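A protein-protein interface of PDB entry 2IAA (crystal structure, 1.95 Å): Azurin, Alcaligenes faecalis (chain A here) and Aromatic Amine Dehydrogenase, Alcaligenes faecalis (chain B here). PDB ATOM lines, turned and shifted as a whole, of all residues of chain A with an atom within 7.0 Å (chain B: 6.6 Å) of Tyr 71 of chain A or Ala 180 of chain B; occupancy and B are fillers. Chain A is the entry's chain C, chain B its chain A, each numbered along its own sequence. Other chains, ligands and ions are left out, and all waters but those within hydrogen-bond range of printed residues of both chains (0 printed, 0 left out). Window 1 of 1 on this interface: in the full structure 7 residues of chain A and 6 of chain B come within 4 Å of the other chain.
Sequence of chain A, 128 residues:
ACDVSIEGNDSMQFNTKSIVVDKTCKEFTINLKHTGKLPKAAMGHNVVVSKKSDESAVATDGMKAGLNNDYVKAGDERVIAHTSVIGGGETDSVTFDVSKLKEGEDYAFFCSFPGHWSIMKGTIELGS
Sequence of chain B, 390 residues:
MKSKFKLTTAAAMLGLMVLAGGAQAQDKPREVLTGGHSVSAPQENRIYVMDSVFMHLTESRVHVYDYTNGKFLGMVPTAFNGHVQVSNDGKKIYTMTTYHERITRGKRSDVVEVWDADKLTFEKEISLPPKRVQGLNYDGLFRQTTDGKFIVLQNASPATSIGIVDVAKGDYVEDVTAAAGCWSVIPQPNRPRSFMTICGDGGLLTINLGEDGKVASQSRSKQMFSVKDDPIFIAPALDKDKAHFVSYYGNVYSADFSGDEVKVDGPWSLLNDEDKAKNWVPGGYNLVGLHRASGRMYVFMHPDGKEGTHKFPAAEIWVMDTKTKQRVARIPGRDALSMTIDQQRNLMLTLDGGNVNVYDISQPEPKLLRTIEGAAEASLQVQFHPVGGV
The side-chain carboxylate (OD2) of Asp 61 of chain A lies within salt-bridge range of the side-chain amino group (NZ) of Lys 64 of chain A (3.8 Å). N of Tyr 71 of chain A lies within hydrogen-bond range of O of Gly 66 of chain A, 2.8 Å away. OG of Ser 112 of chain A sits at hydrogen-bond distance from O of Tyr 71 of chain A, 2.6 Å away. SG of Cys 199 of chain B is disulfide-bonded to SG of Cys 182 of chain B (2.0 Å).
Ala 41 of chain A touches Ala 159 of chain B (O to CB, 3.2 Å). CG of Met 63 of chain A touches O of Ala 180 of chain B, 3.99 Å away. Arg 220 of chain B touches Met 63 of chain A. Lys 64 of chain A touches Arg 220 of chain B (CD to CD, 3.8 Å). Ala 180 of chain B touches Tyr 71 of chain A (CB to OH, 3.7 Å).
Lys 40 of chain A touches none of the printed residues of chain B. Of the printed residues of chain B, Ala 41 of chain A touches Ala 159. Of the printed residues of chain B, Lys 64 of chain A touches Arg 220. Of chain B, only Ala 180 comes within 4 Å of Tyr 71 of chain A. Printed residues of chain A within 4 Å of Ala 159 of chain B: Ala 41 (3.2 Å). Of the printed residues of chain A, Ala 180 of chain B touches Met 63 (3.99 Å) and Tyr 71 (3.7 Å). Cys 199 of chain B touches none of the printed residues of chain A. Printed residues of chain A within 4 Å of Arg 220 of chain B: Met 63 (2.9 Å) and Lys 64 (3.8 Å).
Of the 27 printed residues of chain A, 4 touch a printed residue of chain B. Hydrophobic or aromatic side chains of chain A within 4 Å of the printed part of chain B: Met 63 and Tyr 71. Along chain A the printed residues that touch a printed residue of chain B span positions 41 to 71. Among the printed residues, 5 pairs touch across the chains. Among the printed residues, no Asp or Glu carboxylate lies within 4 Å of a Lys or Arg side-chain nitrogen of the other chain.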
ATOM      1  N   LYS A  40       1.526   7.431 -24.221  1.00  0.00           N
ATOM      2  CA  LYS A  40       1.174   8.812 -23.907  1.00  0.00           C
ATOM      3  C   LYS A  40      -0.331   8.972 -23.731  1.00  0.00           C
ATOM      4  O   LYS A  40      -0.792   9.795 -22.942  1.00  0.00           O
ATOM      5  CB  LYS A  40       1.651   9.763 -25.013  1.00  0.00           C
ATOM      6  CG  LYS A  40       0.875   9.653 -26.318  1.00  0.00           C
ATOM      7  CD  LYS A  40       1.005  10.921 -27.158  1.00  0.00           C
ATOM      8  CE  LYS A  40       2.438  11.172 -27.600  1.00  0.00           C
ATOM      9  NZ  LYS A  40       2.945  10.075 -28.470  1.00  0.00           N
ATOM     10  N   ALA A  41      -1.093   8.176 -24.473  1.00  0.00           N
ATOM     11  CA  ALA A  41      -2.547   8.239 -24.411  1.00  0.00           C
ATOM     12  C   ALA A  41      -3.075   7.853 -23.036  1.00  0.00           C
ATOM     13  O   ALA A  41      -4.161   8.281 -22.644  1.00  0.00           O
ATOM     14  CB  ALA A  41      -3.153   7.329 -25.473  1.00  0.00           C
ATOM     15  N   GLY A  44       0.808  10.072 -20.272  1.00  0.00           N
ATOM     16  CA  GLY A  44       1.753  10.992 -20.881  1.00  0.00           C
ATOM     17  C   GLY A  44       2.199  12.099 -19.942  1.00  0.00           C
ATOM     18  O   GLY A  44       1.500  12.434 -18.984  1.00  0.00           O
ATOM     19  N   ASN A  46       4.488  16.080 -19.707  1.00  0.00           N
ATOM     20  CA  ASN A  46       5.003  17.252 -20.403  1.00  0.00           C
ATOM     21  C   ASN A  46       5.408  18.258 -19.336  1.00  0.00           C
ATOM     22  O   ASN A  46       5.152  18.042 -18.152  1.00  0.00           O
ATOM     23  CB  ASN A  46       3.937  17.846 -21.338  1.00  0.00           C
ATOM     24  CG  ASN A  46       2.905  18.689 -20.606  1.00  0.00           C
ATOM     25  OD1 ASN A  46       2.700  18.544 -19.402  1.00  0.00           O
ATOM     26  ND2 ASN A  46       2.238  19.567 -21.344  1.00  0.00           N
ATOM     27  N   VAL A  48       5.279  22.417 -18.350  1.00  0.00           N
ATOM     28  CA  VAL A  48       4.749  23.740 -18.639  1.00  0.00           C
ATOM     29  C   VAL A  48       5.257  24.735 -17.604  1.00  0.00           C
ATOM     30  O   VAL A  48       5.054  24.552 -16.403  1.00  0.00           O
ATOM     31  CB  VAL A  48       3.205  23.744 -18.609  1.00  0.00           C
ATOM     32  CG1 VAL A  48       2.679  25.140 -18.916  1.00  0.00           C
ATOM     33  CG2 VAL A  48       2.663  22.740 -19.611  1.00  0.00           C
ATOM     34  N   VAL A  58      -3.802  27.692 -16.156  1.00  0.00           N
ATOM     35  CA  VAL A  58      -3.163  27.184 -17.366  1.00  0.00           C
ATOM     36  C   VAL A  58      -3.462  25.695 -17.559  1.00  0.00           C
ATOM     37  O   VAL A  58      -3.776  25.254 -18.665  1.00  0.00           O
ATOM     38  CB  VAL A  58      -1.628  27.393 -17.312  1.00  0.00           C
ATOM     39  CG1 VAL A  58      -0.974  26.785 -18.546  1.00  0.00           C
ATOM     40  CG2 VAL A  58      -1.309  28.877 -17.232  1.00  0.00           C
ATOM     41  N   ALA A  59      -3.366  24.928 -16.476  1.00  0.00           N
ATOM     42  CA  ALA A  59      -3.623  23.492 -16.525  1.00  0.00           C
ATOM     43  C   ALA A  59      -5.066  23.205 -16.928  1.00  0.00           C
ATOM     44  O   ALA A  59      -5.340  22.239 -17.640  1.00  0.00           O
ATOM     45  CB  ALA A  59      -3.326  22.862 -15.166  1.00  0.00           C
ATOM     46  N   ASP A  61      -7.163  25.210 -18.802  1.00  0.00           N
ATOM     47  CA  ASP A  61      -7.356  25.512 -20.215  1.00  0.00           C
ATOM     48  C   ASP A  61      -6.583  24.509 -21.059  1.00  0.00           C
ATOM     49  O   ASP A  61      -7.008  24.148 -22.156  1.00  0.00           O
ATOM     50  CB  ASP A  61      -6.885  26.934 -20.533  1.00  0.00           C
ATOM     51  CG  ASP A  61      -7.776  28.000 -19.915  1.00  0.00           C
ATOM     52  OD1 ASP A  61      -7.516  29.201 -20.145  1.00  0.00           O
ATOM     53  OD2 ASP A  61      -8.735  27.638 -19.202  1.00  0.00           O
ATOM     54  N   GLY A  62      -5.443  24.062 -20.540  1.00  0.00           N
ATOM     55  CA  GLY A  62      -4.636  23.093 -21.258  1.00  0.00           C
ATOM     56  C   GLY A  62      -5.399  21.792 -21.411  1.00  0.00           C
ATOM     57  O   GLY A  62      -5.247  21.082 -22.404  1.00  0.00           O
ATOM     58  N   MET A  63      -6.226  21.485 -20.418  1.00  0.00           N
ATOM     59  CA  MET A  63      -7.035  20.274 -20.434  1.00  0.00           C
ATOM     60  C   MET A  63      -8.092  20.385 -21.527  1.00  0.00           C
ATOM     61  O   MET A  63      -8.443  19.395 -22.168  1.00  0.00           O
ATOM     62  CB  MET A  63      -7.712  20.075 -19.075  1.00  0.00           C
ATOM     63  CG  MET A  63      -8.609  18.850 -19.005  1.00  0.00           C
ATOM     64  SD  MET A  63     -10.282  19.248 -18.458  1.00  0.00           S
ATOM     65  CE  MET A  63     -10.987  19.836 -19.981  1.00  0.00           C
ATOM     66  N   LYS A  64      -8.598  21.599 -21.737  1.00  0.00           N
ATOM     67  CA  LYS A  64      -9.608  21.839 -22.763  1.00  0.00           C
ATOM     68  C   LYS A  64      -8.963  21.898 -24.149  1.00  0.00           C
ATOM     69  O   LYS A  64      -9.630  21.696 -25.162  1.00  0.00           O
ATOM     70  CB  LYS A  64     -10.344  23.155 -22.498  1.00  0.00           C
ATOM     71  CG  LYS A  64     -11.025  23.259 -21.138  1.00  0.00           C
ATOM     72  CD  LYS A  64     -11.895  24.513 -21.080  1.00  0.00           C
ATOM     73  CE  LYS A  64     -12.500  24.731 -19.701  1.00  0.00           C
ATOM     74  NZ  LYS A  64     -11.464  25.077 -18.688  1.00  0.00           N
ATOM     75  N   ALA A  65      -7.663  22.178 -24.183  1.00  0.00           N
ATOM     76  CA  ALA A  65      -6.922  22.267 -25.438  1.00  0.00           C
ATOM     77  C   ALA A  65      -6.810  20.898 -26.108  1.00  0.00           C
ATOM     78  O   ALA A  65      -6.784  20.795 -27.334  1.00  0.00           O
ATOM     79  CB  ALA A  65      -5.532  22.840 -25.183  1.00  0.00           C
ATOM     80  N   GLY A  66      -6.741  19.851 -25.294  1.00  0.00           N
ATOM     81  CA  GLY A  66      -6.643  18.507 -25.830  1.00  0.00           C
ATOM     82  C   GLY A  66      -5.216  18.035 -26.028  1.00  0.00           C
ATOM     83  O   GLY A  66      -4.264  18.797 -25.846  1.00  0.00           O
ATOM     84  N   LEU A  67      -5.073  16.769 -26.407  1.00  0.00           N
ATOM     85  CA  LEU A  67      -3.764  16.173 -26.631  1.00  0.00           C
ATOM     86  C   LEU A  67      -3.093  16.710 -27.889  1.00  0.00           C
ATOM     87  O   LEU A  67      -1.872  16.847 -27.935  1.00  0.00           O
ATOM     88  CB  LEU A  67      -3.889  14.651 -26.737  1.00  0.00           C
ATOM     89  CG  LEU A  67      -2.588  13.892 -27.010  1.00  0.00           C
ATOM     90  CD1 LEU A  67      -1.637  14.069 -25.834  1.00  0.00           C
ATOM     91  CD2 LEU A  67      -2.891  12.422 -27.233  1.00  0.00           C
ATOM     92  N   ASN A  68      -3.891  17.007 -28.913  1.00  0.00           N
ATOM     93  CA  ASN A  68      -3.348  17.528 -30.166  1.00  0.00           C
ATOM     94  C   ASN A  68      -2.676  18.882 -29.978  1.00  0.00           C
ATOM     95  O   ASN A  68      -1.970  19.365 -30.862  1.00  0.00           O
ATOM     96  CB  ASN A  68      -4.450  17.631 -31.224  1.00  0.00           C
ATOM     97  CG  ASN A  68      -4.871  16.274 -31.755  1.00  0.00           C
ATOM     98  OD1 ASN A  68      -4.040  15.493 -32.222  1.00  0.00           O
ATOM     99  ND2 ASN A  68      -6.169  15.988 -31.692  1.00  0.00           N
ATOM    100  N   ASN A  69      -2.902  19.492 -28.821  1.00  0.00           N
ATOM    101  CA  ASN A  69      -2.299  20.779 -28.509  1.00  0.00           C
ATOM    102  C   ASN A  69      -1.353  20.616 -27.324  1.00  0.00           C
ATOM    103  O   ASN A  69      -1.027  21.581 -26.635  1.00  0.00           O
ATOM    104  CB  ASN A  69      -3.383  21.808 -28.184  1.00  0.00           C
ATOM    105  CG  ASN A  69      -4.212  22.178 -29.397  1.00  0.00           C
ATOM    106  OD1 ASN A  69      -3.683  22.662 -30.399  1.00  0.00           O
ATOM    107  ND2 ASN A  69      -5.516  21.950 -29.315  1.00  0.00           N
ATOM    108  N   ASP A  70      -0.917  19.378 -27.103  1.00  0.00           N
ATOM    109  CA  ASP A  70      -0.006  19.052 -26.012  1.00  0.00           C
ATOM    110  C   ASP A  70      -0.558  19.526 -24.672  1.00  0.00           C
ATOM    111  O   ASP A  70       0.195  19.873 -23.760  1.00  0.00           O
ATOM    112  CB  ASP A  70       1.367  19.673 -26.274  1.00  0.00           C
ATOM    113  CG  ASP A  70       2.050  19.073 -27.489  1.00  0.00           C
ATOM    114  OD1 ASP A  70       2.348  17.859 -27.464  1.00  0.00           O
ATOM    115  OD2 ASP A  70       2.282  19.812 -28.470  1.00  0.00           O
ATOM    116  N   TYR A  71      -1.883  19.525 -24.568  1.00  0.00           N
ATOM    117  CA  TYR A  71      -2.577  19.947 -23.360  1.00  0.00           C
ATOM    118  C   TYR A  71      -2.156  21.323 -22.860  1.00  0.00           C
ATOM    119  O   TYR A  71      -1.891  21.515 -21.674  1.00  0.00           O
ATOM    120  CB  TYR A  71      -2.399  18.896 -22.259  1.00  0.00           C
ATOM    121  CG  TYR A  71      -3.260  17.671 -22.479  1.00  0.00           C
ATOM    122  CD1 TYR A  71      -4.651  17.779 -22.538  1.00  0.00           C
ATOM    123  CD2 TYR A  71      -2.689  16.408 -22.651  1.00  0.00           C
ATOM    124  CE1 TYR A  71      -5.453  16.665 -22.762  1.00  0.00           C
ATOM    125  CE2 TYR A  71      -3.486  15.283 -22.877  1.00  0.00           C
ATOM    126  CZ  TYR A  71      -4.868  15.423 -22.932  1.00  0.00           C
ATOM    127  OH  TYR A  71      -5.666  14.327 -23.160  1.00  0.00           O
ATOM    128  N   VAL A  72      -2.106  22.274 -23.787  1.00  0.00           N
ATOM    129  CA  VAL A  72      -1.748  23.656 -23.490  1.00  0.00           C
ATOM    130  C   VAL A  72      -2.512  24.554 -24.458  1.00  0.00           C
ATOM    131  O   VAL A  72      -2.405  24.395 -25.674  1.00  0.00           O
ATOM    132  CB  VAL A  72      -0.235  23.909 -23.679  1.00  0.00           C
ATOM    133  CG1 VAL A  72       0.087  25.369 -23.387  1.00  0.00           C
ATOM    134  CG2 VAL A  72       0.568  22.998 -22.765  1.00  0.00           C
ATOM    135  N   LYS A  73      -3.293  25.486 -23.919  1.00  0.00           N
ATOM    136  CA  LYS A  73      -4.062  26.395 -24.759  1.00  0.00           C
ATOM    137  C   LYS A  73      -3.124  27.117 -25.721  1.00  0.00           C
ATOM    138  O   LYS A  73      -2.160  27.761 -25.303  1.00  0.00           O
ATOM    139  CB  LYS A  73      -4.816  27.410 -23.893  1.00  0.00           C
ATOM    140  CG  LYS A  73      -5.686  28.377 -24.687  1.00  0.00           C
ATOM    141  CD  LYS A  73      -6.502  29.276 -23.766  1.00  0.00           C
ATOM    142  CE  LYS A  73      -5.607  30.129 -22.875  1.00  0.00           C
ATOM    143  NZ  LYS A  73      -6.399  30.994 -21.955  1.00  0.00           N
ATOM    144  N   HIS A  82       6.818  25.462 -22.831  1.00  0.00           N
ATOM    145  CA  HIS A  82       6.228  24.153 -22.594  1.00  0.00           C
ATOM    146  C   HIS A  82       6.718  23.131 -23.616  1.00  0.00           C
ATOM    147  O   HIS A  82       6.989  23.471 -24.770  1.00  0.00           O
ATOM    148  CB  HIS A  82       4.699  24.249 -22.638  1.00  0.00           C
ATOM    149  CG  HIS A  82       4.135  24.365 -24.020  1.00  0.00           C
ATOM    150  ND1 HIS A  82       4.068  23.296 -24.889  1.00  0.00           N
ATOM    151  CD2 HIS A  82       3.605  25.420 -24.683  1.00  0.00           C
ATOM    152  CE1 HIS A  82       3.518  23.687 -26.024  1.00  0.00           C
ATOM    153  NE2 HIS A  82       3.228  24.971 -25.926  1.00  0.00           N
ATOM    154  N   THR A  83       6.827  21.880 -23.180  1.00  0.00           N
ATOM    155  CA  THR A  83       7.281  20.795 -24.045  1.00  0.00           C
ATOM    156  C   THR A  83       6.089  20.054 -24.638  1.00  0.00           C
ATOM    157  O   THR A  83       4.940  20.319 -24.284  1.00  0.00           O
ATOM    158  CB  THR A  83       8.125  19.767 -23.262  1.00  0.00           C
ATOM    159  OG1 THR A  83       7.283  19.058 -22.345  1.00  0.00           O
ATOM    160  CG2 THR A  83       9.227  20.463 -22.478  1.00  0.00           C
ATOM    161  N   VAL A  85       3.837  16.604 -25.313  1.00  0.00           N
ATOM    162  CA  VAL A  85       3.477  15.471 -24.469  1.00  0.00           C
ATOM    163  C   VAL A  85       4.151  14.213 -25.002  1.00  0.00           C
ATOM    164  O   VAL A  85       3.961  13.841 -26.160  1.00  0.00           O
ATOM    165  CB  VAL A  85       1.946  15.250 -24.445  1.00  0.00           C
ATOM    166  CG1 VAL A  85       1.609  14.049 -23.574  1.00  0.00           C
ATOM    167  CG2 VAL A  85       1.247  16.496 -23.919  1.00  0.00           C
ATOM    168  N   CYS A 111       3.023  19.413 -15.076  1.00  0.00           N
ATOM    169  CA  CYS A 111       2.530  18.644 -16.209  1.00  0.00           C
ATOM    170  C   CYS A 111       1.048  18.946 -16.374  1.00  0.00           C
ATOM    171  O   CYS A 111       0.262  18.758 -15.444  1.00  0.00           O
ATOM    172  CB  CYS A 111       2.726  17.148 -15.981  1.00  0.00           C
ATOM    173  SG  CYS A 111       2.240  16.165 -17.415  1.00  0.00           S
ATOM    174  N   SER A 112       0.673  19.419 -17.556  1.00  0.00           N
ATOM    175  CA  SER A 112      -0.715  19.759 -17.827  1.00  0.00           C
ATOM    176  C   SER A 112      -1.546  18.557 -18.268  1.00  0.00           C
ATOM    177  O   SER A 112      -2.743  18.690 -18.521  1.00  0.00           O
ATOM    178  CB  SER A 112      -0.788  20.864 -18.888  1.00  0.00           C
ATOM    179  OG  SER A 112      -0.182  20.456 -20.101  1.00  0.00           O
ATOM    180  N   PHE A 113      -0.918  17.389 -18.365  1.00  0.00           N
ATOM    181  CA  PHE A 113      -1.649  16.191 -18.761  1.00  0.00           C
ATOM    182  C   PHE A 113      -2.732  15.994 -17.702  1.00  0.00           C
ATOM    183  O   PHE A 113      -2.434  15.905 -16.510  1.00  0.00           O
ATOM    184  CB  PHE A 113      -0.712  14.976 -18.814  1.00  0.00           C
ATOM    185  CG  PHE A 113      -1.315  13.773 -19.494  1.00  0.00           C
ATOM    186  CD1 PHE A 113      -2.244  12.970 -18.835  1.00  0.00           C
ATOM    187  CD2 PHE A 113      -0.968  13.456 -20.805  1.00  0.00           C
ATOM    188  CE1 PHE A 113      -2.818  11.868 -19.470  1.00  0.00           C
ATOM    189  CE2 PHE A 113      -1.538  12.358 -21.451  1.00  0.00           C
ATOM    190  CZ  PHE A 113      -2.465  11.562 -20.782  1.00  0.00           C
ATOM    191  N   PRO A 114      -4.005  15.930 -18.130  1.00  0.00           N
ATOM    192  CA  PRO A 114      -5.185  15.759 -17.273  1.00  0.00           C
ATOM    193  C   PRO A 114      -4.989  15.078 -15.914  1.00  0.00           C
ATOM    194  O   PRO A 114      -4.704  13.884 -15.829  1.00  0.00           O
ATOM    195  CB  PRO A 114      -6.145  15.001 -18.184  1.00  0.00           C
ATOM    196  CG  PRO A 114      -5.891  15.664 -19.501  1.00  0.00           C
ATOM    197  CD  PRO A 114      -4.367  15.741 -19.548  1.00  0.00           C
ATOM    198  N   ALA B 159      -6.013   7.541 -17.917  1.00  0.00           N
ATOM    199  CA  ALA B 159      -6.507   8.691 -18.667  1.00  0.00           C
ATOM    200  C   ALA B 159      -7.957   8.346 -18.995  1.00  0.00           C
ATOM    201  O   ALA B 159      -8.255   7.191 -19.326  1.00  0.00           O
ATOM    202  CB  ALA B 159      -5.703   8.877 -19.945  1.00  0.00           C
ATOM    203  N   THR B 160      -8.857   9.323 -18.904  1.00  0.00           N
ATOM    204  CA  THR B 160     -10.266   9.049 -19.173  1.00  0.00           C
ATOM    205  C   THR B 160     -10.766   9.408 -20.570  1.00  0.00           C
ATOM    206  O   THR B 160     -10.248  10.309 -21.225  1.00  0.00           O
ATOM    207  CB  THR B 160     -11.187   9.755 -18.139  1.00  0.00           C
ATOM    208  OG1 THR B 160     -11.204  11.171 -18.383  1.00  0.00           O
ATOM    209  CG2 THR B 160     -10.693   9.492 -16.718  1.00  0.00           C
ATOM    210  N   SER B 161     -11.783   8.677 -21.014  1.00  0.00           N
ATOM    211  CA  SER B 161     -12.411   8.903 -22.307  1.00  0.00           C
ATOM    212  C   SER B 161     -13.723   8.143 -22.288  1.00  0.00           C
ATOM    213  O   SER B 161     -13.956   7.306 -21.414  1.00  0.00           O
ATOM    214  CB  SER B 161     -11.531   8.389 -23.459  1.00  0.00           C
ATOM    215  OG  SER B 161     -11.478   6.970 -23.485  1.00  0.00           O
ATOM    216  N   ILE B 162     -14.585   8.439 -23.248  1.00  0.00           N
ATOM    217  CA  ILE B 162     -15.867   7.768 -23.330  1.00  0.00           C
ATOM    218  C   ILE B 162     -15.922   6.890 -24.572  1.00  0.00           C
ATOM    219  O   ILE B 162     -15.495   7.295 -25.653  1.00  0.00           O
ATOM    220  CB  ILE B 162     -17.013   8.794 -23.334  1.00  0.00           C
ATOM    221  CG1 ILE B 162     -17.096   9.444 -21.946  1.00  0.00           C
ATOM    222  CG2 ILE B 162     -18.327   8.126 -23.727  1.00  0.00           C
ATOM    223  CD1 ILE B 162     -18.148  10.523 -21.818  1.00  0.00           C
ATOM    224  N   VAL B 176     -14.420   8.817 -27.551  1.00  0.00           N
ATOM    225  CA  VAL B 176     -14.500  10.253 -27.304  1.00  0.00           C
ATOM    226  C   VAL B 176     -13.392  10.724 -26.369  1.00  0.00           C
ATOM    227  O   VAL B 176     -13.602  10.878 -25.161  1.00  0.00           O
ATOM    228  CB  VAL B 176     -15.870  10.638 -26.705  1.00  0.00           C
ATOM    229  CG1 VAL B 176     -16.007  12.157 -26.649  1.00  0.00           C
ATOM    230  CG2 VAL B 176     -16.988  10.036 -27.540  1.00  0.00           C
ATOM    231  N   THR B 177     -12.214  10.955 -26.938  1.00  0.00           N
ATOM    232  CA  THR B 177     -11.068  11.409 -26.162  1.00  0.00           C
ATOM    233  C   THR B 177     -11.194  12.877 -25.753  1.00  0.00           C
ATOM    234  O   THR B 177     -10.377  13.386 -24.987  1.00  0.00           O
ATOM    235  CB  THR B 177      -9.743  11.206 -26.939  1.00  0.00           C
ATOM    236  OG1 THR B 177      -9.869  11.742 -28.262  1.00  0.00           O
ATOM    237  CG2 THR B 177      -9.399   9.728 -27.021  1.00  0.00           C
ATOM    238  N   ALA B 178     -12.220  13.553 -26.259  1.00  0.00           N
ATOM    239  CA  ALA B 178     -12.446  14.952 -25.910  1.00  0.00           C
ATOM    240  C   ALA B 178     -12.981  15.017 -24.479  1.00  0.00           C
ATOM    241  O   ALA B 178     -13.054  16.085 -23.879  1.00  0.00           O
ATOM    242  CB  ALA B 178     -13.449  15.579 -26.868  1.00  0.00           C
ATOM    243  N   ALA B 179     -13.351  13.859 -23.938  1.00  0.00           N
ATOM    244  CA  ALA B 179     -13.881  13.784 -22.582  1.00  0.00           C
ATOM    245  C   ALA B 179     -12.780  13.577 -21.542  1.00  0.00           C
ATOM    246  O   ALA B 179     -13.066  13.381 -20.360  1.00  0.00           O
ATOM    247  CB  ALA B 179     -14.918  12.659 -22.487  1.00  0.00           C
ATOM    248  N   ALA B 180     -11.524  13.613 -21.982  1.00  0.00           N
ATOM    249  CA  ALA B 180     -10.392  13.453 -21.074  1.00  0.00           C
ATOM    250  C   ALA B 180     -10.487  14.507 -19.972  1.00  0.00           C
ATOM    251  O   ALA B 180     -10.710  15.688 -20.246  1.00  0.00           O
ATOM    252  CB  ALA B 180      -9.078  13.609 -21.837  1.00  0.00           C
ATOM    253  N   GLY B 181     -10.325  14.082 -18.724  1.00  0.00           N
ATOM    254  CA  GLY B 181     -10.419  15.017 -17.619  1.00  0.00           C
ATOM    255  C   GLY B 181     -11.839  15.144 -17.098  1.00  0.00           C
ATOM    256  O   GLY B 181     -12.099  15.909 -16.170  1.00  0.00           O
ATOM    257  N   CYS B 182     -12.767  14.405 -17.697  1.00  0.00           N
ATOM    258  CA  CYS B 182     -14.163  14.440 -17.266  1.00  0.00           C
ATOM    259  C   CYS B 182     -14.545  13.072 -16.705  1.00  0.00           C
ATOM    260  O   CYS B 182     -13.755  12.129 -16.770  1.00  0.00           O
ATOM    261  CB  CYS B 182     -15.072  14.797 -18.442  1.00  0.00           C
ATOM    262  SG  CYS B 182     -14.540  16.289 -19.343  1.00  0.00           S
ATOM    263  N   CYS B 199     -16.764  17.634 -15.828  1.00  0.00           N
ATOM    264  CA  CYS B 199     -15.326  17.789 -15.994  1.00  0.00           C
ATOM    265  C   CYS B 199     -14.581  18.451 -14.841  1.00  0.00           C
ATOM    266  O   CYS B 199     -15.170  19.138 -14.005  1.00  0.00           O
ATOM    267  CB  CYS B 199     -15.037  18.526 -17.301  1.00  0.00           C
ATOM    268  SG  CYS B 199     -15.831  17.739 -18.742  1.00  0.00           S
ATOM    269  N   GLY B 200     -13.270  18.231 -14.821  1.00  0.00           N
ATOM    270  CA  GLY B 200     -12.419  18.762 -13.773  1.00  0.00           C
ATOM    271  C   GLY B 200     -12.406  20.266 -13.594  1.00  0.00           C
ATOM    272  O   GLY B 200     -11.872  20.756 -12.601  1.00  0.00           O
ATOM    273  N   LEU B 205     -19.453  19.009 -20.129  1.00  0.00           N
ATOM    274  CA  LEU B 205     -19.085  18.841 -21.529  1.00  0.00           C
ATOM    275  C   LEU B 205     -20.215  18.069 -22.204  1.00  0.00           C
ATOM    276  O   LEU B 205     -20.588  16.981 -21.753  1.00  0.00           O
ATOM    277  CB  LEU B 205     -17.782  18.048 -21.650  1.00  0.00           C
ATOM    278  CG  LEU B 205     -17.372  17.660 -23.075  1.00  0.00           C
ATOM    279  CD1 LEU B 205     -16.967  18.909 -23.845  1.00  0.00           C
ATOM    280  CD2 LEU B 205     -16.226  16.664 -23.034  1.00  0.00           C
ATOM    281  N   ARG B 220     -19.157  23.282 -24.334  1.00  0.00           N
ATOM    282  CA  ARG B 220     -18.787  23.338 -22.926  1.00  0.00           C
ATOM    283  C   ARG B 220     -19.558  24.415 -22.189  1.00  0.00           C
ATOM    284  O   ARG B 220     -19.648  25.555 -22.648  1.00  0.00           O
ATOM    285  CB  ARG B 220     -17.293  23.607 -22.772  1.00  0.00           C
ATOM    286  CG  ARG B 220     -16.485  22.378 -22.456  1.00  0.00           C
ATOM    287  CD  ARG B 220     -15.161  22.741 -21.811  1.00  0.00           C
ATOM    288  NE  ARG B 220     -14.533  21.569 -21.213  1.00  0.00           N
ATOM    289  CZ  ARG B 220     -14.063  20.536 -21.902  1.00  0.00           C
ATOM    290  NH1 ARG B 220     -14.137  20.527 -23.227  1.00  0.00           N
ATOM    291  NH2 ARG B 220     -13.535  19.504 -21.263  1.00  0.00           N
